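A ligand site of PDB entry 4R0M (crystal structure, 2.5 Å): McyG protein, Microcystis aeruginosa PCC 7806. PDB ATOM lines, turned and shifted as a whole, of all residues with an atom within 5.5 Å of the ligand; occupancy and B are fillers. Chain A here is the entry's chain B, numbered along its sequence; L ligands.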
ATOM      1  N   THR A 182       9.041 -34.553   5.645  1.00  0.00           N
ATOM      2  CA  THR A 182       8.562 -34.531   4.257  1.00  0.00           C
ATOM      3  C   THR A 182       8.932 -35.849   3.577  1.00  0.00           C
ATOM      4  O   THR A 182       9.990 -36.419   3.866  1.00  0.00           O
ATOM      5  CB  THR A 182       9.188 -33.377   3.458  1.00  0.00           C
ATOM      6  OG1 THR A 182      10.614 -33.406   3.615  1.00  0.00           O
ATOM      7  CG2 THR A 182       8.663 -32.033   3.930  1.00  0.00           C
ATOM      8  N   HIS A 226       0.919 -29.242   7.824  1.00  0.00           N
ATOM      9  CA  HIS A 226       1.819 -28.608   6.872  1.00  0.00           C
ATOM     10  C   HIS A 226       2.411 -27.316   7.379  1.00  0.00           C
ATOM     11  O   HIS A 226       1.759 -26.574   8.118  1.00  0.00           O
ATOM     12  CB  HIS A 226       1.117 -28.384   5.546  1.00  0.00           C
ATOM     13  CG  HIS A 226       2.047 -28.023   4.423  1.00  0.00           C
ATOM     14  ND1 HIS A 226       2.326 -26.742   4.113  1.00  0.00           N
ATOM     15  CD2 HIS A 226       2.777 -28.815   3.548  1.00  0.00           C
ATOM     16  CE1 HIS A 226       3.190 -26.717   3.081  1.00  0.00           C
ATOM     17  NE2 HIS A 226       3.464 -27.988   2.735  1.00  0.00           N
ATOM     18  N   VAL A 227       3.645 -27.041   6.975  1.00  0.00           N
ATOM     19  CA  VAL A 227       4.417 -25.880   7.449  1.00  0.00           C
ATOM     20  C   VAL A 227       3.754 -24.511   7.177  1.00  0.00           C
ATOM     21  O   VAL A 227       3.924 -23.578   7.961  1.00  0.00           O
ATOM     22  CB  VAL A 227       5.858 -25.910   6.892  1.00  0.00           C
ATOM     23  CG1 VAL A 227       5.899 -25.591   5.398  1.00  0.00           C
ATOM     24  CG2 VAL A 227       6.775 -24.969   7.672  1.00  0.00           C
ATOM     25  N   GLY A 228       2.986 -24.419   6.091  1.00  0.00           N
ATOM     26  CA  GLY A 228       2.289 -23.194   5.726  1.00  0.00           C
ATOM     27  C   GLY A 228       1.169 -22.845   6.674  1.00  0.00           C
ATOM     28  O   GLY A 228       0.877 -21.670   6.906  1.00  0.00           O
ATOM     29  N   PHE A 232       3.156 -19.750   8.701  1.00  0.00           N
ATOM     30  CA  PHE A 232       2.675 -18.548   8.009  1.00  0.00           C
ATOM     31  C   PHE A 232       1.265 -18.122   8.441  1.00  0.00           C
ATOM     32  O   PHE A 232       0.993 -16.920   8.585  1.00  0.00           O
ATOM     33  CB  PHE A 232       2.748 -18.733   6.483  1.00  0.00           C
ATOM     34  CG  PHE A 232       2.160 -17.587   5.691  1.00  0.00           C
ATOM     35  CD1 PHE A 232       2.621 -16.278   5.876  1.00  0.00           C
ATOM     36  CD2 PHE A 232       1.170 -17.828   4.752  1.00  0.00           C
ATOM     37  CE1 PHE A 232       2.073 -15.227   5.142  1.00  0.00           C
ATOM     38  CE2 PHE A 232       0.627 -16.774   4.010  1.00  0.00           C
ATOM     39  CZ  PHE A 232       1.081 -15.485   4.209  1.00  0.00           C
ATOM     40  N   TRP A 272      -4.145 -18.069   1.688  1.00  0.00           N
ATOM     41  CA  TRP A 272      -3.232 -18.871   0.871  1.00  0.00           C
ATOM     42  C   TRP A 272      -3.830 -20.163   0.386  1.00  0.00           C
ATOM     43  O   TRP A 272      -4.633 -20.800   1.072  1.00  0.00           O
ATOM     44  CB  TRP A 272      -1.926 -19.130   1.653  1.00  0.00           C
ATOM     45  CG  TRP A 272      -1.151 -20.356   1.220  1.00  0.00           C
ATOM     46  CD1 TRP A 272      -0.527 -20.579  -0.013  1.00  0.00           C
ATOM     47  CD2 TRP A 272      -0.866 -21.555   2.018  1.00  0.00           C
ATOM     48  NE1 TRP A 272       0.095 -21.802  -0.028  1.00  0.00           N
ATOM     49  CE2 TRP A 272      -0.080 -22.439   1.151  1.00  0.00           C
ATOM     50  CE3 TRP A 272      -1.184 -21.972   3.303  1.00  0.00           C
ATOM     51  CZ2 TRP A 272       0.365 -23.682   1.580  1.00  0.00           C
ATOM     52  CZ3 TRP A 272      -0.735 -23.227   3.729  1.00  0.00           C
ATOM     53  CH2 TRP A 272       0.018 -24.060   2.889  1.00  0.00           C
ATOM     54  N   VAL A 302      -1.885 -15.409  -1.239  1.00  0.00           N
ATOM     55  CA  VAL A 302      -0.725 -16.203  -1.617  1.00  0.00           C
ATOM     56  C   VAL A 302      -1.068 -17.386  -2.524  1.00  0.00           C
ATOM     57  O   VAL A 302      -1.917 -18.208  -2.192  1.00  0.00           O
ATOM     58  CB  VAL A 302       0.043 -16.690  -0.375  1.00  0.00           C
ATOM     59  CG1 VAL A 302       1.335 -17.401  -0.762  1.00  0.00           C
ATOM     60  CG2 VAL A 302       0.343 -15.524   0.548  1.00  0.00           C
ATOM     61  N   ASN A 303      -0.411 -17.422  -3.683  1.00  0.00           N
ATOM     62  CA  ASN A 303      -0.358 -18.604  -4.523  1.00  0.00           C
ATOM     63  C   ASN A 303       1.019 -19.230  -4.325  1.00  0.00           C
ATOM     64  O   ASN A 303       2.011 -18.697  -4.816  1.00  0.00           O
ATOM     65  CB  ASN A 303      -0.599 -18.239  -5.994  1.00  0.00           C
ATOM     66  CG  ASN A 303      -0.735 -19.455  -6.901  1.00  0.00           C
ATOM     67  OD1 ASN A 303      -0.095 -20.490  -6.689  1.00  0.00           O
ATOM     68  ND2 ASN A 303      -1.576 -19.333  -7.919  1.00  0.00           N
ATOM     69  N   ALA A 304       1.064 -20.324  -3.578  1.00  0.00           N
ATOM     70  CA  ALA A 304       2.326 -21.000  -3.248  1.00  0.00           C
ATOM     71  C   ALA A 304       2.119 -22.467  -2.873  1.00  0.00           C
ATOM     72  O   ALA A 304       1.026 -22.857  -2.458  1.00  0.00           O
ATOM     73  CB  ALA A 304       3.056 -20.264  -2.133  1.00  0.00           C
ATOM     74  N   GLY A 305       3.176 -23.256  -3.001  1.00  0.00           N
ATOM     75  CA  GLY A 305       3.113 -24.688  -2.724  1.00  0.00           C
ATOM     76  C   GLY A 305       3.445 -25.542  -3.928  1.00  0.00           C
ATOM     77  O   GLY A 305       3.933 -26.662  -3.781  1.00  0.00           O
ATOM     78  N   GLU A 306       3.173 -25.000  -5.120  1.00  0.00           N
ATOM     79  CA  GLU A 306       3.458 -25.670  -6.386  1.00  0.00           C
ATOM     80  C   GLU A 306       3.641 -24.623  -7.475  1.00  0.00           C
ATOM     81  O   GLU A 306       3.375 -23.437  -7.259  1.00  0.00           O
ATOM     82  CB  GLU A 306       2.341 -26.640  -6.765  1.00  0.00           C
ATOM     83  CG  GLU A 306       1.013 -25.986  -7.107  1.00  0.00           C
ATOM     84  CD  GLU A 306      -0.064 -26.972  -7.531  1.00  0.00           C
ATOM     85  OE1 GLU A 306      -1.220 -26.538  -7.713  1.00  0.00           O
ATOM     86  OE2 GLU A 306       0.227 -28.179  -7.665  1.00  0.00           O
ATOM     87  N   GLN A 307       4.091 -25.061  -8.642  1.00  0.00           N
ATOM     88  CA  GLN A 307       4.298 -24.189  -9.790  1.00  0.00           C
ATOM     89  C   GLN A 307       3.061 -23.340 -10.058  1.00  0.00           C
ATOM     90  O   GLN A 307       1.941 -23.839 -10.040  1.00  0.00           O
ATOM     91  CB  GLN A 307       4.692 -25.009 -11.029  1.00  0.00           C
ATOM     92  CG  GLN A 307       5.276 -24.180 -12.165  1.00  0.00           C
ATOM     93  CD  GLN A 307       6.659 -23.634 -11.880  1.00  0.00           C
ATOM     94  OE1 GLN A 307       7.476 -24.278 -11.208  1.00  0.00           O
ATOM     95  NE2 GLN A 307       6.940 -22.446 -12.413  1.00  0.00           N
ATOM     96  N   VAL A 308       3.289 -22.047 -10.293  1.00  0.00           N
ATOM     97  CA  VAL A 308       2.208 -21.088 -10.531  1.00  0.00           C
ATOM     98  C   VAL A 308       1.969 -20.948 -12.035  1.00  0.00           C
ATOM     99  O   VAL A 308       2.903 -20.722 -12.803  1.00  0.00           O
ATOM    100  CB  VAL A 308       2.518 -19.699  -9.906  1.00  0.00           C
ATOM    101  CG1 VAL A 308       1.344 -18.747 -10.066  1.00  0.00           C
ATOM    102  CG2 VAL A 308       2.885 -19.849  -8.429  1.00  0.00           C
ATOM    103  N   ALA A 333       4.380 -16.790  -4.315  1.00  0.00           N
ATOM    104  CA  ALA A 333       5.506 -16.843  -3.381  1.00  0.00           C
ATOM    105  C   ALA A 333       6.229 -18.175  -3.455  1.00  0.00           C
ATOM    106  O   ALA A 333       5.660 -19.178  -3.888  1.00  0.00           O
ATOM    107  CB  ALA A 333       5.015 -16.586  -1.966  1.00  0.00           C
ATOM    108  N   PHE A 334       7.489 -18.189  -3.033  1.00  0.00           N
ATOM    109  CA  PHE A 334       8.211 -19.433  -2.859  1.00  0.00           C
ATOM    110  C   PHE A 334       8.488 -19.715  -1.380  1.00  0.00           C
ATOM    111  O   PHE A 334       8.827 -18.806  -0.617  1.00  0.00           O
ATOM    112  CB  PHE A 334       9.522 -19.446  -3.649  1.00  0.00           C
ATOM    113  CG  PHE A 334      10.325 -20.701  -3.468  1.00  0.00           C
ATOM    114  CD1 PHE A 334       9.999 -21.866  -4.158  1.00  0.00           C
ATOM    115  CD2 PHE A 334      11.407 -20.734  -2.601  1.00  0.00           C
ATOM    116  CE1 PHE A 334      10.734 -23.030  -3.992  1.00  0.00           C
ATOM    117  CE2 PHE A 334      12.142 -21.893  -2.422  1.00  0.00           C
ATOM    118  CZ  PHE A 334      11.810 -23.036  -3.118  1.00  0.00           C
ATOM    119  N   GLY A 335       8.325 -20.974  -1.003  1.00  0.00           N
ATOM    120  CA  GLY A 335       8.653 -21.424   0.336  1.00  0.00           C
ATOM    121  C   GLY A 335       8.754 -22.944   0.389  1.00  0.00           C
ATOM    122  O   GLY A 335       8.418 -23.623  -0.586  1.00  0.00           O
ATOM    123  N   MET A 336       9.233 -23.458   1.519  1.00  0.00           N
ATOM    124  CA  MET A 336       9.351 -24.899   1.728  1.00  0.00           C
ATOM    125  C   MET A 336       9.388 -25.156   3.209  1.00  0.00           C
ATOM    126  O   MET A 336       9.524 -24.229   4.007  1.00  0.00           O
ATOM    127  CB  MET A 336      10.580 -25.471   1.026  1.00  0.00           C
ATOM    128  CG  MET A 336      11.908 -24.847   1.448  1.00  0.00           C
ATOM    129  SD  MET A 336      13.238 -25.082   0.017  1.00  0.00           S
ATOM    130  CE  MET A 336      13.170 -27.049  -0.159  1.00  0.00           C
ATOM    131  N   THR A 337       9.265 -26.432   3.578  1.00  0.00           N
ATOM    132  CA  THR A 337       9.370 -26.851   4.969  1.00  0.00           C
ATOM    133  C   THR A 337      10.718 -26.439   5.563  1.00  0.00           C
ATOM    134  O   THR A 337      10.792 -26.014   6.720  1.00  0.00           O
ATOM    135  CB  THR A 337       9.173 -28.374   5.102  1.00  0.00           C
ATOM    136  OG1 THR A 337       7.927 -28.745   4.488  1.00  0.00           O
ATOM    137  CG2 THR A 337       9.153 -28.814   6.558  1.00  0.00           C
ATOM    138  N   GLU A 338      11.765 -26.535   4.752  1.00  0.00           N
ATOM    139  CA  GLU A 338      13.125 -26.223   5.162  1.00  0.00           C
ATOM    140  C   GLU A 338      13.355 -24.742   5.492  1.00  0.00           C
ATOM    141  O   GLU A 338      14.357 -24.392   6.135  1.00  0.00           O
ATOM    142  CB  GLU A 338      14.128 -26.697   4.102  1.00  0.00           C
ATOM    143  CG  GLU A 338      14.357 -28.209   4.088  1.00  0.00           C
ATOM    144  CD  GLU A 338      13.350 -28.985   3.249  1.00  0.00           C
ATOM    145  OE1 GLU A 338      12.327 -28.401   2.825  1.00  0.00           O
ATOM    146  OE2 GLU A 338      13.579 -30.192   3.015  1.00  0.00           O
ATOM    147  N   SER A 341       8.079 -22.382   5.601  1.00  0.00           N
ATOM    148  CA  SER A 341       7.210 -21.862   4.535  1.00  0.00           C
ATOM    149  C   SER A 341       7.851 -20.668   3.800  1.00  0.00           C
ATOM    150  O   SER A 341       9.048 -20.707   3.490  1.00  0.00           O
ATOM    151  CB  SER A 341       5.768 -21.578   5.012  1.00  0.00           C
ATOM    152  OG  SER A 341       5.675 -20.370   5.739  1.00  0.00           O
ATOM    153  N   GLY A 342       7.060 -19.634   3.520  1.00  0.00           N
ATOM    154  CA  GLY A 342       7.471 -18.509   2.666  1.00  0.00           C
ATOM    155  C   GLY A 342       8.836 -17.899   2.918  1.00  0.00           C
ATOM    156  O   GLY A 342       9.180 -17.584   4.055  1.00  0.00           O
ATOM    157  N   ILE A 343       9.623 -17.751   1.854  1.00  0.00           N
ATOM    158  CA  ILE A 343      10.951 -17.135   1.925  1.00  0.00           C
ATOM    159  C   ILE A 343      11.114 -15.986   0.917  1.00  0.00           C
ATOM    160  O   ILE A 343      11.890 -15.055   1.147  1.00  0.00           O
ATOM    161  CB  ILE A 343      12.093 -18.165   1.796  1.00  0.00           C
ATOM    162  CG1 ILE A 343      13.439 -17.544   2.191  1.00  0.00           C
ATOM    163  CG2 ILE A 343      12.137 -18.775   0.397  1.00  0.00           C
ATOM    164  CD1 ILE A 343      14.560 -18.541   2.413  1.00  0.00           C
ATOM    165  N   TRP A 345       8.541 -13.285  -1.542  1.00  0.00           N
ATOM    166  CA  TRP A 345       7.179 -12.801  -1.728  1.00  0.00           C
ATOM    167  C   TRP A 345       7.112 -11.851  -2.885  1.00  0.00           C
ATOM    168  O   TRP A 345       7.945 -10.957  -3.009  1.00  0.00           O
ATOM    169  CB  TRP A 345       6.670 -12.103  -0.461  1.00  0.00           C
ATOM    170  CG  TRP A 345       6.757 -12.944   0.791  1.00  0.00           C
ATOM    171  CD1 TRP A 345       7.774 -12.949   1.741  1.00  0.00           C
ATOM    172  CD2 TRP A 345       5.786 -13.942   1.260  1.00  0.00           C
ATOM    173  NE1 TRP A 345       7.503 -13.838   2.743  1.00  0.00           N
ATOM    174  CE2 TRP A 345       6.328 -14.479   2.518  1.00  0.00           C
ATOM    175  CE3 TRP A 345       4.571 -14.434   0.800  1.00  0.00           C
ATOM    176  CZ2 TRP A 345       5.671 -15.444   3.254  1.00  0.00           C
ATOM    177  CZ3 TRP A 345       3.912 -15.412   1.554  1.00  0.00           C
ATOM    178  CH2 TRP A 345       4.453 -15.909   2.742  1.00  0.00           C
ATOM    179  N   LEU A 363       8.100 -14.953  -8.309  1.00  0.00           N
ATOM    180  CA  LEU A 363       7.831 -15.301  -6.915  1.00  0.00           C
ATOM    181  C   LEU A 363       8.489 -14.300  -5.969  1.00  0.00           C
ATOM    182  O   LEU A 363       8.589 -14.523  -4.759  1.00  0.00           O
ATOM    183  CB  LEU A 363       8.275 -16.743  -6.621  1.00  0.00           C
ATOM    184  CG  LEU A 363       7.743 -17.854  -7.537  1.00  0.00           C
ATOM    185  CD1 LEU A 363       8.228 -19.215  -7.072  1.00  0.00           C
ATOM    186  CD2 LEU A 363       6.218 -17.855  -7.654  1.00  0.00           C
ATOM    187  N   THR A 419      17.945 -26.598  -2.544  1.00  0.00           N
ATOM    188  CA  THR A 419      16.509 -26.837  -2.433  1.00  0.00           C
ATOM    189  C   THR A 419      16.042 -28.024  -3.280  1.00  0.00           C
ATOM    190  O   THR A 419      15.008 -28.636  -2.997  1.00  0.00           O
ATOM    191  CB  THR A 419      15.706 -25.599  -2.845  1.00  0.00           C
ATOM    192  OG1 THR A 419      15.847 -25.372  -4.256  1.00  0.00           O
ATOM    193  CG2 THR A 419      16.191 -24.355  -2.088  1.00  0.00           C
ATOM    194  N   ASP A 421      15.323 -27.398  -6.362  1.00  0.00           N
ATOM    195  CA  ASP A 421      14.486 -26.680  -7.313  1.00  0.00           C
ATOM    196  C   ASP A 421      15.300 -25.985  -8.390  1.00  0.00           C
ATOM    197  O   ASP A 421      16.457 -25.604  -8.174  1.00  0.00           O
ATOM    198  CB  ASP A 421      13.595 -25.666  -6.591  1.00  0.00           C
ATOM    199  CG  ASP A 421      12.494 -26.321  -5.770  1.00  0.00           C
ATOM    200  OD1 ASP A 421      11.718 -27.109  -6.349  1.00  0.00           O
ATOM    201  OD2 ASP A 421      12.413 -26.043  -4.558  1.00  0.00           O
ATOM    202  N   ILE A 432      10.781 -19.725 -10.402  1.00  0.00           N
ATOM    203  CA  ILE A 432      10.934 -21.182 -10.414  1.00  0.00           C
ATOM    204  C   ILE A 432      10.453 -21.731 -11.759  1.00  0.00           C
ATOM    205  O   ILE A 432       9.385 -21.356 -12.235  1.00  0.00           O
ATOM    206  CB  ILE A 432      10.202 -21.863  -9.218  1.00  0.00           C
ATOM    207  CG1 ILE A 432      10.823 -21.450  -7.872  1.00  0.00           C
ATOM    208  CG2 ILE A 432      10.178 -23.380  -9.364  1.00  0.00           C
ATOM    209  CD1 ILE A 432      12.275 -21.850  -7.682  1.00  0.00           C
ATOM    210  N   ARG A 435      11.564 -28.665 -11.129  1.00  0.00           N
ATOM    211  CA  ARG A 435      12.249 -29.387 -10.061  1.00  0.00           C
ATOM    212  C   ARG A 435      13.242 -30.391 -10.654  1.00  0.00           C
ATOM    213  O   ARG A 435      12.978 -30.987 -11.700  1.00  0.00           O
ATOM    214  CB  ARG A 435      11.245 -30.080  -9.134  1.00  0.00           C
ATOM    215  CG  ARG A 435      11.877 -30.888  -8.023  1.00  0.00           C
ATOM    216  CD  ARG A 435      11.024 -30.957  -6.779  1.00  0.00           C
ATOM    217  NE  ARG A 435      11.753 -31.597  -5.687  1.00  0.00           N
ATOM    218  CZ  ARG A 435      12.536 -30.964  -4.820  1.00  0.00           C
ATOM    219  NH1 ARG A 435      12.688 -29.639  -4.878  1.00  0.00           N
ATOM    220  NH2 ARG A 435      13.162 -31.655  -3.874  1.00  0.00           N
ATOM    221  N   THR A 529       0.516 -34.776  -1.547  1.00  0.00           N
ATOM    222  CA  THR A 529       0.957 -34.279  -0.249  1.00  0.00           C
ATOM    223  C   THR A 529      -0.268 -33.743   0.478  1.00  0.00           C
ATOM    224  O   THR A 529      -1.318 -33.551  -0.152  1.00  0.00           O
ATOM    225  CB  THR A 529       2.008 -33.158  -0.381  1.00  0.00           C
ATOM    226  OG1 THR A 529       1.461 -32.068  -1.148  1.00  0.00           O
ATOM    227  CG2 THR A 529       3.279 -33.661  -1.041  1.00  0.00           C
ATOM    228  N   ILE A 531      -1.160 -30.928   1.300  1.00  0.00           N
ATOM    229  CA  ILE A 531      -1.684 -29.695   0.707  1.00  0.00           C
ATOM    230  C   ILE A 531      -2.277 -29.848  -0.712  1.00  0.00           C
ATOM    231  O   ILE A 531      -2.742 -28.868  -1.289  1.00  0.00           O
ATOM    232  CB  ILE A 531      -0.643 -28.544   0.743  1.00  0.00           C
ATOM    233  CG1 ILE A 531       0.629 -28.888  -0.036  1.00  0.00           C
ATOM    234  CG2 ILE A 531      -0.357 -28.148   2.178  1.00  0.00           C
ATOM    235  CD1 ILE A 531       1.500 -27.691  -0.333  1.00  0.00           C
ATOM    236  N   LYS A 533      -0.706 -31.186  -3.532  1.00  0.00           N
ATOM    237  CA  LYS A 533       0.255 -31.189  -4.617  1.00  0.00           C
ATOM    238  C   LYS A 533       0.520 -32.626  -5.063  1.00  0.00           C
ATOM    239  O   LYS A 533       0.973 -33.461  -4.271  1.00  0.00           O
ATOM    240  CB  LYS A 533       1.564 -30.520  -4.187  1.00  0.00           C
ATOM    241  CG  LYS A 533       2.671 -30.569  -5.228  1.00  0.00           C
ATOM    242  CD  LYS A 533       3.945 -29.877  -4.747  1.00  0.00           C
ATOM    243  CE  LYS A 533       4.671 -30.679  -3.676  1.00  0.00           C
ATOM    244  NZ  LYS A 533       5.994 -30.089  -3.332  1.00  0.00           N
HETATM  245  C1  LIG L   1       5.512 -26.519   0.693  1.00  0.00           C
HETATM  246  O1  LIG L   1       4.791 -26.990  -0.180  1.00  0.00           O
HETATM  247  C2  LIG L   1       5.668 -25.026   0.809  1.00  0.00           C
HETATM  248  N1  LIG L   1       6.015 -24.589  -0.524  1.00  0.00           N
HETATM  249  C3  LIG L   1       4.379 -24.327   1.243  1.00  0.00           C
HETATM  250  C4  LIG L   1       4.331 -22.793   1.277  1.00  0.00           C
HETATM  251  C5  LIG L   1       5.244 -21.969   0.625  1.00  0.00           C
HETATM  252  C6  LIG L   1       3.292 -22.173   1.991  1.00  0.00           C
HETATM  253  C7  LIG L   1       5.140 -20.579   0.689  1.00  0.00           C
HETATM  254  C8  LIG L   1       3.175 -20.780   2.061  1.00  0.00           C
HETATM  255  C9  LIG L   1       4.100 -19.975   1.407  1.00  0.00           C
HETATM  256  P1  LIG L   1       6.974 -28.771   1.076  1.00  0.00           P
HETATM  257  O2  LIG L   1       6.000 -29.922   1.081  1.00  0.00           O
HETATM  258  O3  LIG L   1       8.250 -28.903   1.857  1.00  0.00           O
HETATM  259  O4  LIG L   1       6.207 -27.442   1.583  1.00  0.00           O
HETATM  260  O5  LIG L   1       7.348 -28.512  -0.477  1.00  0.00           O
HETATM  261  C10 LIG L   1       8.301 -27.529  -0.877  1.00  0.00           C
HETATM  262  C11 LIG L   1       8.448 -27.614  -2.391  1.00  0.00           C
HETATM  263  O6  LIG L   1       7.248 -27.231  -3.069  1.00  0.00           O
HETATM  264  C12 LIG L   1       9.515 -26.686  -2.931  1.00  0.00           C
HETATM  265  O7  LIG L   1      10.820 -27.230  -2.804  1.00  0.00           O
HETATM  266  C13 LIG L   1       9.096 -26.541  -4.379  1.00  0.00           C
HETATM  267  O8  LIG L   1       9.579 -27.646  -5.150  1.00  0.00           O
HETATM  268  C14 LIG L   1       7.583 -26.614  -4.321  1.00  0.00           C
HETATM  269  N2  LIG L   1       7.037 -25.238  -4.382  1.00  0.00           N
HETATM  270  C15 LIG L   1       6.574 -24.528  -3.343  1.00  0.00           C
HETATM  271  N3  LIG L   1       6.133 -23.297  -3.725  1.00  0.00           N
HETATM  272  C16 LIG L   1       6.325 -23.206  -5.049  1.00  0.00           C
HETATM  273  C17 LIG L   1       6.090 -22.184  -6.103  1.00  0.00           C
HETATM  274  N4  LIG L   1       5.540 -20.984  -5.805  1.00  0.00           N
HETATM  275  N5  LIG L   1       6.429 -22.489  -7.381  1.00  0.00           N
HETATM  276  C18 LIG L   1       6.977 -23.684  -7.703  1.00  0.00           C
HETATM  277  N6  LIG L   1       7.214 -24.658  -6.803  1.00  0.00           N
HETATM  278  C19 LIG L   1       6.917 -24.483  -5.478  1.00  0.00           C
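The side-chain carboxylate of Asp 421 lies within hydrogen-bond range of an oxygen (O8) of the ligand (2.5 Å).
O4 of the ligand is in hydrogen-bond range of NE2 of His 226 (3.0 Å).
NZ of Lys 533 lies within hydrogen-bond range of O6 of the ligand, 3.1 Å away.
N1 of the ligand lies within hydrogen-bond range of O of Gly 335 (2.6 Å).
An oxygen (O3) of the ligand lies within hydrogen-bond range of the side-chain hydroxyl (OG1) of Thr 337, 2.7 Å away.
N of Gly 305 lies within hydrogen-bond range of N3 of the ligand (3.0 Å).
O of Ala 333 is in hydrogen-bond range of N4 of the ligand (2.6 Å).
N of Thr 337 lies within hydrogen-bond range of O3 of the ligand (3.2 Å).
O of Asn 303 sits at hydrogen-bond distance from N of Ala 333.
A ring nitrogen (ND1) of His 226 is in hydrogen-bond range of the backbone NH of Gly 228 (3.1 Å).
The backbone carbonyl oxygen (O) of Phe 334 sits at hydrogen-bond distance from the backbone NH (N) of Ile 343 (2.8 Å).
N of Trp 345 lies within hydrogen-bond range of O of Leu 363, at 3.4 Å.
O of Thr 419 sits at hydrogen-bond distance from NH1 of Arg 435, 3.2 Å away.
The backbone carbonyl oxygen (O) of Met 336 lies within hydrogen-bond range of the backbone NH (N) of Ser 341 (2.8 Å).
O of Ile 432 lies within hydrogen-bond range of NE2 of Gln 307, 2.7 Å away.
The backbone NH (N) of Asp 421 sits at hydrogen-bond distance from the side-chain hydroxyl (OG1) of Thr 419 (3.0 Å).
O of Glu 306 lies close to N5 of the ligand, at 3.2 Å.
Thr 182 touches the ligand (CG2 to O3, 3.8 Å).
Gly 228 touches the ligand.
Trp 272 touches the ligand.
Ala 304 touches the ligand.
N of Gln 307 touches C18 of the ligand, at 3.3 Å.
Val 308 touches the ligand (CG2 to N4, 3.9 Å).
Phe 334 touches the ligand.
Met 336 touches the ligand (CE to O7, 3.5 Å).
Ser 341 touches the ligand.
Gly 342 touches the ligand (N to C7, 3.5 Å).
CD1 of Leu 363 touches N4 of the ligand (3.5 Å).
Ile 432 touches the ligand (CG2 to C18, 3.6 Å).
Arg 435 touches the ligand (NH1 to O7, 3.7 Å).
Ile 531 touches the ligand.
Hydrophobic or aromatic side chains within 4 Å of the ligand: His 226, Trp 272, Ala 304, Val 308, Phe 334, Met 336, Leu 363, Ile 432 and Ile 531.
Of the 31 residues printed, 22 come within 4 Å of the ligand.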
